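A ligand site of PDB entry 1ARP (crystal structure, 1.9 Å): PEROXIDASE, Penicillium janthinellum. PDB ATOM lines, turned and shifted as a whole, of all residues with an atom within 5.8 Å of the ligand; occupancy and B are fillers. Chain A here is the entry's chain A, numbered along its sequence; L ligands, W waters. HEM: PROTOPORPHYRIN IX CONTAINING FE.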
ATOM      1  N   SER A  45      15.727   1.547   1.240  1.00  0.00           N
ATOM      2  CA  SER A  45      14.411   1.908   1.721  1.00  0.00           C
ATOM      3  C   SER A  45      13.221   1.381   0.904  1.00  0.00           C
ATOM      4  O   SER A  45      12.292   0.968   1.573  1.00  0.00           O
ATOM      5  CB  SER A  45      14.365   3.447   1.853  1.00  0.00           C
ATOM      6  OG  SER A  45      13.129   3.998   2.313  1.00  0.00           O
ATOM      7  N   VAL A  47      12.544  -1.469  -0.447  1.00  0.00           N
ATOM      8  CA  VAL A  47      12.321  -2.878  -0.053  1.00  0.00           C
ATOM      9  C   VAL A  47      11.687  -2.868   1.330  1.00  0.00           C
ATOM     10  O   VAL A  47      10.680  -3.534   1.555  1.00  0.00           O
ATOM     11  CB  VAL A  47      13.641  -3.692   0.007  1.00  0.00           C
ATOM     12  CG1 VAL A  47      13.352  -5.092   0.459  1.00  0.00           C
ATOM     13  CG2 VAL A  47      14.308  -3.765  -1.350  1.00  0.00           C
ATOM     14  N   ARG A  48      12.302  -2.119   2.261  1.00  0.00           N
ATOM     15  CA  ARG A  48      11.790  -1.988   3.614  1.00  0.00           C
ATOM     16  C   ARG A  48      10.350  -1.449   3.666  1.00  0.00           C
ATOM     17  O   ARG A  48       9.530  -2.020   4.363  1.00  0.00           O
ATOM     18  CB  ARG A  48      12.684  -1.082   4.388  1.00  0.00           C
ATOM     19  CG  ARG A  48      14.083  -1.577   4.556  1.00  0.00           C
ATOM     20  CD  ARG A  48      14.660  -0.756   5.664  1.00  0.00           C
ATOM     21  NE  ARG A  48      15.934  -0.396   5.213  1.00  0.00           N
ATOM     22  CZ  ARG A  48      16.333   0.816   4.909  1.00  0.00           C
ATOM     23  NH1 ARG A  48      15.643   1.939   5.006  1.00  0.00           N
ATOM     24  NH2 ARG A  48      17.482   0.791   4.286  1.00  0.00           N
ATOM     25  N   LYS A  49      10.006  -0.406   2.915  1.00  0.00           N
ATOM     26  CA  LYS A  49       8.661   0.129   2.844  1.00  0.00           C
ATOM     27  C   LYS A  49       7.757  -0.957   2.271  1.00  0.00           C
ATOM     28  O   LYS A  49       6.679  -1.150   2.825  1.00  0.00           O
ATOM     29  CB  LYS A  49       8.559   1.320   1.903  1.00  0.00           C
ATOM     30  CG  LYS A  49       9.294   2.588   2.247  1.00  0.00           C
ATOM     31  CD  LYS A  49       8.726   3.229   3.489  1.00  0.00           C
ATOM     32  CE  LYS A  49       9.622   4.354   3.869  1.00  0.00           C
ATOM     33  NZ  LYS A  49       9.059   5.010   5.012  1.00  0.00           N
ATOM     34  N   LEU A  51       7.914  -4.310   2.424  1.00  0.00           N
ATOM     35  CA  LEU A  51       7.746  -5.314   3.451  1.00  0.00           C
ATOM     36  C   LEU A  51       6.718  -4.850   4.476  1.00  0.00           C
ATOM     37  O   LEU A  51       5.929  -5.651   4.979  1.00  0.00           O
ATOM     38  CB  LEU A  51       9.072  -5.563   4.131  1.00  0.00           C
ATOM     39  CG  LEU A  51      10.125  -6.409   3.400  1.00  0.00           C
ATOM     40  CD1 LEU A  51      11.332  -6.642   4.290  1.00  0.00           C
ATOM     41  CD2 LEU A  51       9.556  -7.783   3.099  1.00  0.00           C
ATOM     42  N   ARG A  52       6.726  -3.558   4.860  1.00  0.00           N
ATOM     43  CA  ARG A  52       5.719  -3.005   5.784  1.00  0.00           C
ATOM     44  C   ARG A  52       4.397  -3.011   5.069  1.00  0.00           C
ATOM     45  O   ARG A  52       3.415  -3.479   5.639  1.00  0.00           O
ATOM     46  CB  ARG A  52       5.944  -1.563   6.146  1.00  0.00           C
ATOM     47  CG  ARG A  52       6.852  -1.257   7.271  1.00  0.00           C
ATOM     48  CD  ARG A  52       6.918   0.274   7.451  1.00  0.00           C
ATOM     49  NE  ARG A  52       5.754   0.850   8.099  1.00  0.00           N
ATOM     50  CZ  ARG A  52       5.498   2.152   8.035  1.00  0.00           C
ATOM     51  NH1 ARG A  52       6.286   3.008   7.386  1.00  0.00           N
ATOM     52  NH2 ARG A  52       4.412   2.622   8.658  1.00  0.00           N
ATOM     53  N   VAL A  54       3.191  -5.070   2.709  1.00  0.00           N
ATOM     54  CA  VAL A  54       2.577  -6.359   2.472  1.00  0.00           C
ATOM     55  C   VAL A  54       1.888  -6.859   3.744  1.00  0.00           C
ATOM     56  O   VAL A  54       0.811  -7.458   3.695  1.00  0.00           O
ATOM     57  CB  VAL A  54       3.709  -7.244   1.926  1.00  0.00           C
ATOM     58  CG1 VAL A  54       4.647  -7.784   3.021  1.00  0.00           C
ATOM     59  CG2 VAL A  54       3.045  -8.322   1.115  1.00  0.00           C
ATOM     60  N   PHE A  55       2.486  -6.578   4.915  1.00  0.00           N
ATOM     61  CA  PHE A  55       1.914  -6.930   6.215  1.00  0.00           C
ATOM     62  C   PHE A  55       0.689  -6.046   6.415  1.00  0.00           C
ATOM     63  O   PHE A  55      -0.376  -6.606   6.634  1.00  0.00           O
ATOM     64  CB  PHE A  55       2.912  -6.666   7.340  1.00  0.00           C
ATOM     65  CG  PHE A  55       2.416  -6.890   8.768  1.00  0.00           C
ATOM     66  CD1 PHE A  55       1.632  -7.952   9.114  1.00  0.00           C
ATOM     67  CD2 PHE A  55       2.779  -5.998   9.757  1.00  0.00           C
ATOM     68  CE1 PHE A  55       1.219  -8.116  10.415  1.00  0.00           C
ATOM     69  CE2 PHE A  55       2.374  -6.176  11.064  1.00  0.00           C
ATOM     70  CZ  PHE A  55       1.584  -7.238  11.402  1.00  0.00           C
ATOM     71  N   HIS A  56       0.709  -4.714   6.281  1.00  0.00           N
ATOM     72  CA  HIS A  56      -0.469  -3.864   6.535  1.00  0.00           C
ATOM     73  C   HIS A  56      -1.602  -4.062   5.552  1.00  0.00           C
ATOM     74  O   HIS A  56      -2.792  -3.766   5.805  1.00  0.00           O
ATOM     75  CB  HIS A  56      -0.017  -2.395   6.550  1.00  0.00           C
ATOM     76  CG  HIS A  56       0.882  -2.017   7.721  1.00  0.00           C
ATOM     77  ND1 HIS A  56       1.398  -0.745   7.951  1.00  0.00           N
ATOM     78  CD2 HIS A  56       1.381  -2.899   8.678  1.00  0.00           C
ATOM     79  CE1 HIS A  56       2.222  -0.877   8.988  1.00  0.00           C
ATOM     80  NE2 HIS A  56       2.245  -2.096   9.427  1.00  0.00           N
ATOM     81  N   PRO A 154      -1.362  -4.449  14.290  1.00  0.00           N
ATOM     82  CA  PRO A 154      -0.697  -4.366  15.568  1.00  0.00           C
ATOM     83  C   PRO A 154       0.141  -3.102  15.635  1.00  0.00           C
ATOM     84  O   PRO A 154       0.840  -2.807  14.666  1.00  0.00           O
ATOM     85  CB  PRO A 154       0.174  -5.598  15.660  1.00  0.00           C
ATOM     86  CG  PRO A 154      -0.549  -6.608  14.859  1.00  0.00           C
ATOM     87  CD  PRO A 154      -1.088  -5.749  13.697  1.00  0.00           C
ATOM     88  N   GLY A 155       0.163  -2.444  16.783  1.00  0.00           N
ATOM     89  CA  GLY A 155       0.951  -1.261  17.017  1.00  0.00           C
ATOM     90  C   GLY A 155       2.122  -1.569  17.940  1.00  0.00           C
ATOM     91  O   GLY A 155       2.061  -2.479  18.778  1.00  0.00           O
ATOM     92  N   PRO A 156       3.205  -0.798  17.899  1.00  0.00           N
ATOM     93  CA  PRO A 156       4.427  -0.972  18.694  1.00  0.00           C
ATOM     94  C   PRO A 156       4.286  -0.748  20.170  1.00  0.00           C
ATOM     95  O   PRO A 156       5.144  -1.119  20.970  1.00  0.00           O
ATOM     96  CB  PRO A 156       5.394  -0.022  18.070  1.00  0.00           C
ATOM     97  CG  PRO A 156       4.503   1.117  17.664  1.00  0.00           C
ATOM     98  CD  PRO A 156       3.317   0.369  17.049  1.00  0.00           C
ATOM     99  N   ILE A 163      -1.194  -8.189  20.598  1.00  0.00           N
ATOM    100  CA  ILE A 163      -0.558  -8.607  19.344  1.00  0.00           C
ATOM    101  C   ILE A 163      -0.920 -10.074  19.103  1.00  0.00           C
ATOM    102  O   ILE A 163      -1.390 -10.370  18.006  1.00  0.00           O
ATOM    103  CB  ILE A 163       0.977  -8.449  19.468  1.00  0.00           C
ATOM    104  CG1 ILE A 163       1.292  -6.983  19.710  1.00  0.00           C
ATOM    105  CG2 ILE A 163       1.673  -8.934  18.203  1.00  0.00           C
ATOM    106  CD1 ILE A 163       2.781  -6.729  20.032  1.00  0.00           C
ATOM    107  N   MET A 167      -3.113 -11.243  15.775  1.00  0.00           N
ATOM    108  CA  MET A 167      -2.458 -12.106  14.797  1.00  0.00           C
ATOM    109  C   MET A 167      -3.146 -13.452  14.786  1.00  0.00           C
ATOM    110  O   MET A 167      -3.345 -14.054  13.739  1.00  0.00           O
ATOM    111  CB  MET A 167      -0.978 -12.291  15.138  1.00  0.00           C
ATOM    112  CG  MET A 167      -0.121 -10.999  15.016  1.00  0.00           C
ATOM    113  SD  MET A 167      -0.181 -10.266  13.370  1.00  0.00           S
ATOM    114  CE  MET A 167       1.286 -11.006  12.726  1.00  0.00           C
ATOM    115  N   VAL A 177       4.010 -15.705  14.627  1.00  0.00           N
ATOM    116  CA  VAL A 177       4.187 -14.267  14.845  1.00  0.00           C
ATOM    117  C   VAL A 177       5.682 -14.053  14.976  1.00  0.00           C
ATOM    118  O   VAL A 177       6.206 -13.160  14.292  1.00  0.00           O
ATOM    119  CB  VAL A 177       3.472 -13.766  16.127  1.00  0.00           C
ATOM    120  CG1 VAL A 177       3.824 -12.290  16.403  1.00  0.00           C
ATOM    121  CG2 VAL A 177       1.990 -13.944  15.957  1.00  0.00           C
ATOM    122  N   LEU A 180       7.337 -14.400  11.413  1.00  0.00           N
ATOM    123  CA  LEU A 180       6.998 -13.290  10.548  1.00  0.00           C
ATOM    124  C   LEU A 180       7.899 -12.057  10.828  1.00  0.00           C
ATOM    125  O   LEU A 180       8.306 -11.282   9.942  1.00  0.00           O
ATOM    126  CB  LEU A 180       5.530 -13.046  10.820  1.00  0.00           C
ATOM    127  CG  LEU A 180       4.533 -12.754   9.771  1.00  0.00           C
ATOM    128  CD1 LEU A 180       4.653 -13.667   8.545  1.00  0.00           C
ATOM    129  CD2 LEU A 180       3.199 -12.891  10.482  1.00  0.00           C
ATOM    130  N   LEU A 181       8.278 -11.943  12.089  1.00  0.00           N
ATOM    131  CA  LEU A 181       9.100 -10.862  12.535  1.00  0.00           C
ATOM    132  C   LEU A 181      10.515 -10.926  12.025  1.00  0.00           C
ATOM    133  O   LEU A 181      11.281  -9.976  12.298  1.00  0.00           O
ATOM    134  CB  LEU A 181       9.096 -10.806  14.043  1.00  0.00           C
ATOM    135  CG  LEU A 181       8.622  -9.561  14.785  1.00  0.00           C
ATOM    136  CD1 LEU A 181       8.297  -8.398  13.867  1.00  0.00           C
ATOM    137  CD2 LEU A 181       7.402  -9.951  15.550  1.00  0.00           C
ATOM    138  N   ALA A 183      11.336 -10.215   9.259  1.00  0.00           N
ATOM    139  CA  ALA A 183      11.395  -9.033   8.442  1.00  0.00           C
ATOM    140  C   ALA A 183      11.966  -7.822   9.160  1.00  0.00           C
ATOM    141  O   ALA A 183      12.457  -6.903   8.503  1.00  0.00           O
ATOM    142  CB  ALA A 183      10.033  -8.690   7.992  1.00  0.00           C
ATOM    143  N   HIS A 184      12.007  -7.757  10.494  1.00  0.00           N
ATOM    144  CA  HIS A 184      12.623  -6.631  11.147  1.00  0.00           C
ATOM    145  C   HIS A 184      14.156  -6.740  11.093  1.00  0.00           C
ATOM    146  O   HIS A 184      14.931  -5.918  11.574  1.00  0.00           O
ATOM    147  CB  HIS A 184      12.110  -6.542  12.595  1.00  0.00           C
ATOM    148  CG  HIS A 184      10.784  -5.814  12.795  1.00  0.00           C
ATOM    149  ND1 HIS A 184      10.316  -5.339  14.006  1.00  0.00           N
ATOM    150  CD2 HIS A 184       9.885  -5.489  11.791  1.00  0.00           C
ATOM    151  CE1 HIS A 184       9.160  -4.709  13.753  1.00  0.00           C
ATOM    152  NE2 HIS A 184       8.887  -4.783  12.504  1.00  0.00           N
ATOM    153  N   LEU A 186      15.486  -6.459   8.157  1.00  0.00           N
ATOM    154  CA  LEU A 186      15.782  -5.588   7.047  1.00  0.00           C
ATOM    155  C   LEU A 186      15.009  -4.349   7.427  1.00  0.00           C
ATOM    156  O   LEU A 186      14.088  -3.950   6.708  1.00  0.00           O
ATOM    157  CB  LEU A 186      15.251  -6.294   5.842  1.00  0.00           C
ATOM    158  CG  LEU A 186      16.124  -7.037   4.801  1.00  0.00           C
ATOM    159  CD1 LEU A 186      17.433  -7.506   5.368  1.00  0.00           C
ATOM    160  CD2 LEU A 186      15.290  -8.172   4.247  1.00  0.00           C
ATOM    161  N   ALA A 187      15.381  -3.659   8.479  1.00  0.00           N
ATOM    162  CA  ALA A 187      14.481  -2.607   8.949  1.00  0.00           C
ATOM    163  C   ALA A 187      14.972  -1.382   9.670  1.00  0.00           C
ATOM    164  O   ALA A 187      16.045  -1.464  10.273  1.00  0.00           O
ATOM    165  CB  ALA A 187      13.451  -3.236   9.859  1.00  0.00           C
ATOM    166  N   SER A 188      14.178  -0.322   9.673  1.00  0.00           N
ATOM    167  CA  SER A 188      14.471   0.889  10.395  1.00  0.00           C
ATOM    168  C   SER A 188      13.144   1.560  10.758  1.00  0.00           C
ATOM    169  O   SER A 188      12.050   1.034  10.562  1.00  0.00           O
ATOM    170  CB  SER A 188      15.341   1.836   9.551  1.00  0.00           C
ATOM    171  OG  SER A 188      14.749   2.394   8.404  1.00  0.00           O
ATOM    172  N   GLN A 189      13.181   2.730  11.386  1.00  0.00           N
ATOM    173  CA  GLN A 189      11.991   3.466  11.773  1.00  0.00           C
ATOM    174  C   GLN A 189      12.242   4.887  11.274  1.00  0.00           C
ATOM    175  O   GLN A 189      13.401   5.353  11.240  1.00  0.00           O
ATOM    176  CB  GLN A 189      11.823   3.426  13.294  1.00  0.00           C
ATOM    177  CG  GLN A 189      12.937   4.070  14.108  1.00  0.00           C
ATOM    178  CD  GLN A 189      12.799   5.562  14.362  1.00  0.00           C
ATOM    179  OE1 GLN A 189      11.715   6.142  14.260  1.00  0.00           O
ATOM    180  NE2 GLN A 189      13.872   6.257  14.678  1.00  0.00           N
ATOM    181  N   GLU A 190      11.194   5.608  10.910  1.00  0.00           N
ATOM    182  CA  GLU A 190      11.331   6.979  10.473  1.00  0.00           C
ATOM    183  C   GLU A 190      10.410   7.882  11.285  1.00  0.00           C
ATOM    184  O   GLU A 190      10.707   9.064  11.511  1.00  0.00           O
ATOM    185  CB  GLU A 190      10.981   7.082   9.033  1.00  0.00           C
ATOM    186  CG  GLU A 190      11.932   6.430   8.067  1.00  0.00           C
ATOM    187  CD  GLU A 190      11.580   6.583   6.575  1.00  0.00           C
ATOM    188  OE1 GLU A 190      10.574   7.170   6.138  1.00  0.00           O
ATOM    189  OE2 GLU A 190      12.385   6.083   5.800  1.00  0.00           O
ATOM    190  N   GLY A 191       9.302   7.316  11.768  1.00  0.00           N
ATOM    191  CA  GLY A 191       8.325   8.103  12.500  1.00  0.00           C
ATOM    192  C   GLY A 191       8.125   7.768  13.963  1.00  0.00           C
ATOM    193  O   GLY A 191       7.190   8.256  14.599  1.00  0.00           O
ATOM    194  N   LEU A 192       8.924   6.898  14.563  1.00  0.00           N
ATOM    195  CA  LEU A 192       8.771   6.606  15.985  1.00  0.00           C
ATOM    196  C   LEU A 192       9.712   7.550  16.703  1.00  0.00           C
ATOM    197  O   LEU A 192       9.451   7.967  17.814  1.00  0.00           O
ATOM    198  CB  LEU A 192       9.119   5.137  16.172  1.00  0.00           C
ATOM    199  CG  LEU A 192       8.014   4.130  16.545  1.00  0.00           C
ATOM    200  CD1 LEU A 192       6.679   4.493  15.925  1.00  0.00           C
ATOM    201  CD2 LEU A 192       8.554   2.743  16.201  1.00  0.00           C
ATOM    202  N   LEU A 201      17.005  -1.497  13.013  1.00  0.00           N
ATOM    203  CA  LEU A 201      16.530  -2.293  14.132  1.00  0.00           C
ATOM    204  C   LEU A 201      17.536  -3.429  14.397  1.00  0.00           C
ATOM    205  O   LEU A 201      17.451  -4.092  15.423  1.00  0.00           O
ATOM    206  CB  LEU A 201      15.123  -2.769  13.797  1.00  0.00           C
ATOM    207  CG  LEU A 201      13.935  -1.889  14.245  1.00  0.00           C
ATOM    208  CD1 LEU A 201      14.269  -0.425  14.311  1.00  0.00           C
ATOM    209  CD2 LEU A 201      12.826  -2.084  13.268  1.00  0.00           C
ATOM    210  N   MET A 243      12.223  -1.026  19.497  1.00  0.00           N
ATOM    211  CA  MET A 243      10.835  -0.738  19.818  1.00  0.00           C
ATOM    212  C   MET A 243      10.293  -1.752  20.855  1.00  0.00           C
ATOM    213  O   MET A 243      10.684  -2.929  20.970  1.00  0.00           O
ATOM    214  CB  MET A 243       9.912  -0.736  18.538  1.00  0.00           C
ATOM    215  CG  MET A 243       9.697  -1.996  17.736  1.00  0.00           C
ATOM    216  SD  MET A 243       8.911  -1.744  16.116  1.00  0.00           S
ATOM    217  CE  MET A 243       7.429  -2.223  16.807  1.00  0.00           C
ATOM    218  N   SER A 245       7.297  -3.379  21.324  1.00  0.00           N
ATOM    219  CA  SER A 245       6.752  -4.685  21.039  1.00  0.00           C
ATOM    220  C   SER A 245       7.783  -5.750  20.735  1.00  0.00           C
ATOM    221  O   SER A 245       7.621  -6.872  21.227  1.00  0.00           O
ATOM    222  CB  SER A 245       5.805  -4.560  19.884  1.00  0.00           C
ATOM    223  OG  SER A 245       6.445  -4.078  18.736  1.00  0.00           O
ATOM    224  N   ASP A 246       8.874  -5.443  19.993  1.00  0.00           N
ATOM    225  CA  ASP A 246       9.954  -6.398  19.748  1.00  0.00           C
ATOM    226  C   ASP A 246      10.646  -6.725  21.040  1.00  0.00           C
ATOM    227  O   ASP A 246      10.997  -7.874  21.229  1.00  0.00           O
ATOM    228  CB  ASP A 246      11.056  -5.900  18.832  1.00  0.00           C
ATOM    229  CG  ASP A 246      10.664  -5.673  17.385  1.00  0.00           C
ATOM    230  OD1 ASP A 246       9.666  -6.213  16.932  1.00  0.00           O
ATOM    231  OD2 ASP A 246      11.383  -4.963  16.707  1.00  0.00           O
ATOM    232  N   LEU A 249       8.157  -9.141  23.149  1.00  0.00           N
ATOM    233  CA  LEU A 249       8.033 -10.414  22.466  1.00  0.00           C
ATOM    234  C   LEU A 249       9.273 -11.266  22.598  1.00  0.00           C
ATOM    235  O   LEU A 249       9.161 -12.479  22.690  1.00  0.00           O
ATOM    236  CB  LEU A 249       7.717 -10.205  20.980  1.00  0.00           C
ATOM    237  CG  LEU A 249       6.321  -9.710  20.597  1.00  0.00           C
ATOM    238  CD1 LEU A 249       6.306  -9.222  19.171  1.00  0.00           C
ATOM    239  CD2 LEU A 249       5.357 -10.835  20.795  1.00  0.00           C
ATOM    240  N   TYR A 273      10.446 -18.237   7.957  1.00  0.00           N
ATOM    241  CA  TYR A 273       9.958 -16.981   7.432  1.00  0.00           C
ATOM    242  C   TYR A 273       9.221 -17.266   6.157  1.00  0.00           C
ATOM    243  O   TYR A 273       8.069 -16.858   6.054  1.00  0.00           O
ATOM    244  CB  TYR A 273      11.109 -16.014   7.153  1.00  0.00           C
ATOM    245  CG  TYR A 273      10.661 -14.685   6.565  1.00  0.00           C
ATOM    246  CD1 TYR A 273       9.985 -13.773   7.361  1.00  0.00           C
ATOM    247  CD2 TYR A 273      10.944 -14.370   5.255  1.00  0.00           C
ATOM    248  CE1 TYR A 273       9.593 -12.540   6.860  1.00  0.00           C
ATOM    249  CE2 TYR A 273      10.565 -13.147   4.743  1.00  0.00           C
ATOM    250  CZ  TYR A 273       9.895 -12.235   5.546  1.00  0.00           C
ATOM    251  OH  TYR A 273       9.520 -10.998   5.044  1.00  0.00           O
ATOM    252  N   MET A 277       5.226 -16.274   5.554  1.00  0.00           N
ATOM    253  CA  MET A 277       4.912 -15.336   4.486  1.00  0.00           C
ATOM    254  C   MET A 277       4.023 -15.952   3.433  1.00  0.00           C
ATOM    255  O   MET A 277       3.162 -15.265   2.920  1.00  0.00           O
ATOM    256  CB  MET A 277       6.156 -14.831   3.765  1.00  0.00           C
ATOM    257  CG  MET A 277       6.926 -13.903   4.647  1.00  0.00           C
ATOM    258  SD  MET A 277       6.056 -12.340   4.797  1.00  0.00           S
ATOM    259  CE  MET A 277       6.585 -11.504   3.336  1.00  0.00           C
ATOM    260  N   MET A 280       0.566 -15.859   4.794  1.00  0.00           N
ATOM    261  CA  MET A 280       0.077 -14.507   4.867  1.00  0.00           C
ATOM    262  C   MET A 280      -0.261 -13.935   3.510  1.00  0.00           C
ATOM    263  O   MET A 280      -1.172 -13.114   3.410  1.00  0.00           O
ATOM    264  CB  MET A 280       1.132 -13.607   5.580  1.00  0.00           C
ATOM    265  CG  MET A 280       0.642 -12.145   5.743  1.00  0.00           C
ATOM    266  SD  MET A 280       1.698 -10.942   6.580  1.00  0.00           S
ATOM    267  CE  MET A 280       2.845 -10.765   5.247  1.00  0.00           C
HETATM  268  CHA HEM L   1       9.122  -1.210  10.641  1.00  0.00           C
HETATM  269  CHB HEM L   1       5.829  -2.298  13.954  1.00  0.00           C
HETATM  270  CHC HEM L   1       5.624  -6.794  12.218  1.00  0.00           C
HETATM  271  CHD HEM L   1       8.201  -5.400   8.462  1.00  0.00           C
HETATM  272  C1A HEM L   1       8.260  -1.121  11.717  1.00  0.00           C
HETATM  273  C2A HEM L   1       8.010   0.064  12.451  1.00  0.00           C
HETATM  274  C3A HEM L   1       7.019  -0.206  13.329  1.00  0.00           C
HETATM  275  C4A HEM L   1       6.686  -1.576  13.153  1.00  0.00           C
HETATM  276  CMA HEM L   1       6.337   0.739  14.303  1.00  0.00           C
HETATM  277  CAA HEM L   1       8.716   1.385  12.180  1.00  0.00           C
HETATM  278  CBA HEM L   1       7.959   2.251  11.157  1.00  0.00           C
HETATM  279  CGA HEM L   1       8.504   3.648  11.025  1.00  0.00           C
HETATM  280  O1A HEM L   1       9.163   3.937  10.052  1.00  0.00           O
HETATM  281  O2A HEM L   1       8.296   4.474  11.905  1.00  0.00           O
HETATM  282  C1B HEM L   1       5.594  -3.669  13.878  1.00  0.00           C
HETATM  283  C2B HEM L   1       4.794  -4.459  14.830  1.00  0.00           C
HETATM  284  C3B HEM L   1       4.784  -5.747  14.368  1.00  0.00           C
HETATM  285  C4B HEM L   1       5.590  -5.747  13.139  1.00  0.00           C
HETATM  286  CMB HEM L   1       4.068  -3.930  16.053  1.00  0.00           C
HETATM  287  CAB HEM L   1       3.973  -6.793  14.830  1.00  0.00           C
HETATM  288  CBB HEM L   1       4.407  -7.819  15.742  1.00  0.00           C
HETATM  289  C1C HEM L   1       6.202  -6.769  10.990  1.00  0.00           C
HETATM  290  C2C HEM L   1       6.005  -7.795   9.980  1.00  0.00           C
HETATM  291  C3C HEM L   1       6.661  -7.352   8.870  1.00  0.00           C
HETATM  292  C4C HEM L   1       7.289  -6.093   9.243  1.00  0.00           C
HETATM  293  CMC HEM L   1       5.221  -9.091  10.171  1.00  0.00           C
HETATM  294  CAC HEM L   1       6.626  -7.833   7.569  1.00  0.00           C
HETATM  295  CBC HEM L   1       6.715  -9.189   7.088  1.00  0.00           C
HETATM  296  C1D HEM L   1       8.789  -4.195   8.804  1.00  0.00           C
HETATM  297  C2D HEM L   1       9.819  -3.544   8.054  1.00  0.00           C
HETATM  298  C3D HEM L   1      10.061  -2.364   8.675  1.00  0.00           C
HETATM  299  C4D HEM L   1       9.215  -2.308   9.803  1.00  0.00           C
HETATM  300  CMD HEM L   1      10.539  -4.097   6.849  1.00  0.00           C
HETATM  301  CAD HEM L   1      11.092  -1.306   8.312  1.00  0.00           C
HETATM  302  CBD HEM L   1      10.611  -0.235   7.374  1.00  0.00           C
HETATM  303  CGD HEM L   1      11.590   0.861   7.041  1.00  0.00           C
HETATM  304  O1D HEM L   1      11.192   1.819   6.420  1.00  0.00           O
HETATM  305  O2D HEM L   1      12.751   0.794   7.367  1.00  0.00           O
HETATM  306  NA  HEM L   1       7.434  -2.142  12.138  1.00  0.00           N
HETATM  307  NB  HEM L   1       6.115  -4.489  12.883  1.00  0.00           N
HETATM  308  NC  HEM L   1       6.944  -5.712  10.509  1.00  0.00           N
HETATM  309  ND  HEM L   1       8.468  -3.464   9.919  1.00  0.00           N
HETATM  310 FE   HEM L   1       7.285  -3.980  11.414  1.00  0.00          FE
HETATM  311  O   HOH W   1       4.348   2.612  12.205  1.00  0.00           O
HETATM  312  O   HOH W   2       7.493   5.997   8.561  1.00  0.00           O
HETATM  313  O   HOH W   3       7.002  -6.036  16.913  1.00  0.00           O
HETATM  314  O   HOH W   4       2.723  -2.878  12.412  1.00  0.00           O
HETATM  315  O   HOH W   5       5.673   4.796  12.885  1.00  0.00           O
HETATM  316  O   HOH W   6       4.699  -0.020  10.875  1.00  0.00           O
HETATM  317  O   HOH W   7       9.106   3.091   7.514  1.00  0.00           O
HETATM  318  O   HOH W   8       4.756  -2.669  10.604  1.00  0.00           O
HETATM  319  O   HOH W   9      12.939   3.228   5.071  1.00  0.00           O
HETATM  320  O   HOH W  10       2.908  -0.873  14.126  1.00  0.00           O
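The backbone NH (N) of Leu 192 is in hydrogen-bond range of the side-chain amide oxygen (OE1) of Gln 189 (2.9 Å).
The side-chain carboxylate (OD2) of Asp 246 is in hydrogen-bond range of a ring nitrogen (ND1) of His 184, 2.9 Å away.
The backbone carbonyl oxygen of Ala 187 is in hydrogen-bond range of the backbone NH of Leu 201, 2.9 Å away.
The backbone NH (N) of Ser 245 is in hydrogen-bond range of the backbone carbonyl oxygen (O) of Pro 156, 3.1 Å away.
The side-chain sulfur (SD) of Met 277 sits close to the side-chain hydroxyl (OH) of Tyr 273, 3.7 Å away.
OE1 of Glu 190 is in salt-bridge range of NZ of Lys 49 (2.9 Å).
Water W9 lies within hydrogen-bond range of O1D of the ligand (2.6 Å), OG of Ser 45 (2.9 Å), NH1 of Arg 48 (3.0 Å) and OE2 of Glu 190 (3.0 Å).
Water W7 lies within hydrogen-bond range of O1A of the ligand, NH1 of Arg 52 and NZ of Lys 49.
Water W2 lies within hydrogen-bond range of an oxygen (O1A) of the ligand (3.0 Å) and the guanidinium group of Arg 52 (3.4 Å).
Water W4 lies within hydrogen-bond range of O of Pro 154 (2.9 Å) and NE2 of His 56 (3.1 Å).
Water W3 bridges OD1 of Asp 246 and OG of Ser 245.
An oxygen (O2D) of the ligand lies within salt-bridge range of the guanidinium group (NH1) of Arg 48.
O1A of the ligand sits at hydrogen-bond distance from N of Glu 190.
FE of the ligand is bound by NE2 of His 184, at 2.1 Å.
N of Gly 191 lies within hydrogen-bond range of O2A of the ligand, 3.0 Å away.
The backbone NH (N) of Ser 188 sits at hydrogen-bond distance from an oxygen (O2D) of the ligand (2.9 Å).
The side-chain hydroxyl (OG) of Ser 188 sits at hydrogen-bond distance from an oxygen (O2D) of the ligand, 2.8 Å away.
CE of Lys 49 touches O1D of the ligand (3.9 Å).
CB of Leu 51 touches CMD of the ligand (3.4 Å).
Arg 52 touches the ligand (CG to C4D, 3.6 Å).
Phe 55 touches the ligand (CE2 to CHC, 3.5 Å).
Pro 154 touches the ligand (O to CMB, 3.7 Å).
Gly 155 touches the ligand.
Pro 156 touches the ligand (N to CMB, 3.7 Å).
Ile 163 touches the ligand.
Leu 180 touches the ligand.
Leu 181 touches the ligand (CD1 to CHC, 3.5 Å).
CB of Ala 183 touches CBC of the ligand, 3.5 Å away.
Leu 186 touches the ligand.
CB of Ala 187 touches CAD of the ligand, 3.4 Å away.
Gln 189 touches the ligand (CA to O1A, 3.3 Å).
Leu 192 touches the ligand (CD2 to CMA, 3.5 Å).
CE of Met 243 touches CHB of the ligand, at 3.3 Å.
Ser 245 touches the ligand.
OH of Tyr 273 touches CBC of the ligand, 3.9 Å away.
Met 277 touches the ligand.
Hydrophobic or aromatic side chains within 4 Å of the ligand: Leu 51, Phe 55, Pro 156, Ile 163, Leu 180, Leu 181, Ala 183, His 184, Ala 187, Leu 192, Met 243 and Met 277.
Within 4 Å of the ligand: Arg 48, Lys 49, Leu 51, Arg 52, Phe 55, Pro 154, Gly 155, Pro 156, Ile 163, Leu 180, Leu 181, Ala 183, His 184, Leu 186, Ala 187, Ser 188, Gln 189, Glu 190, Gly 191, Leu 192, Met 243, Ser 245, Tyr 273 and Met 277.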
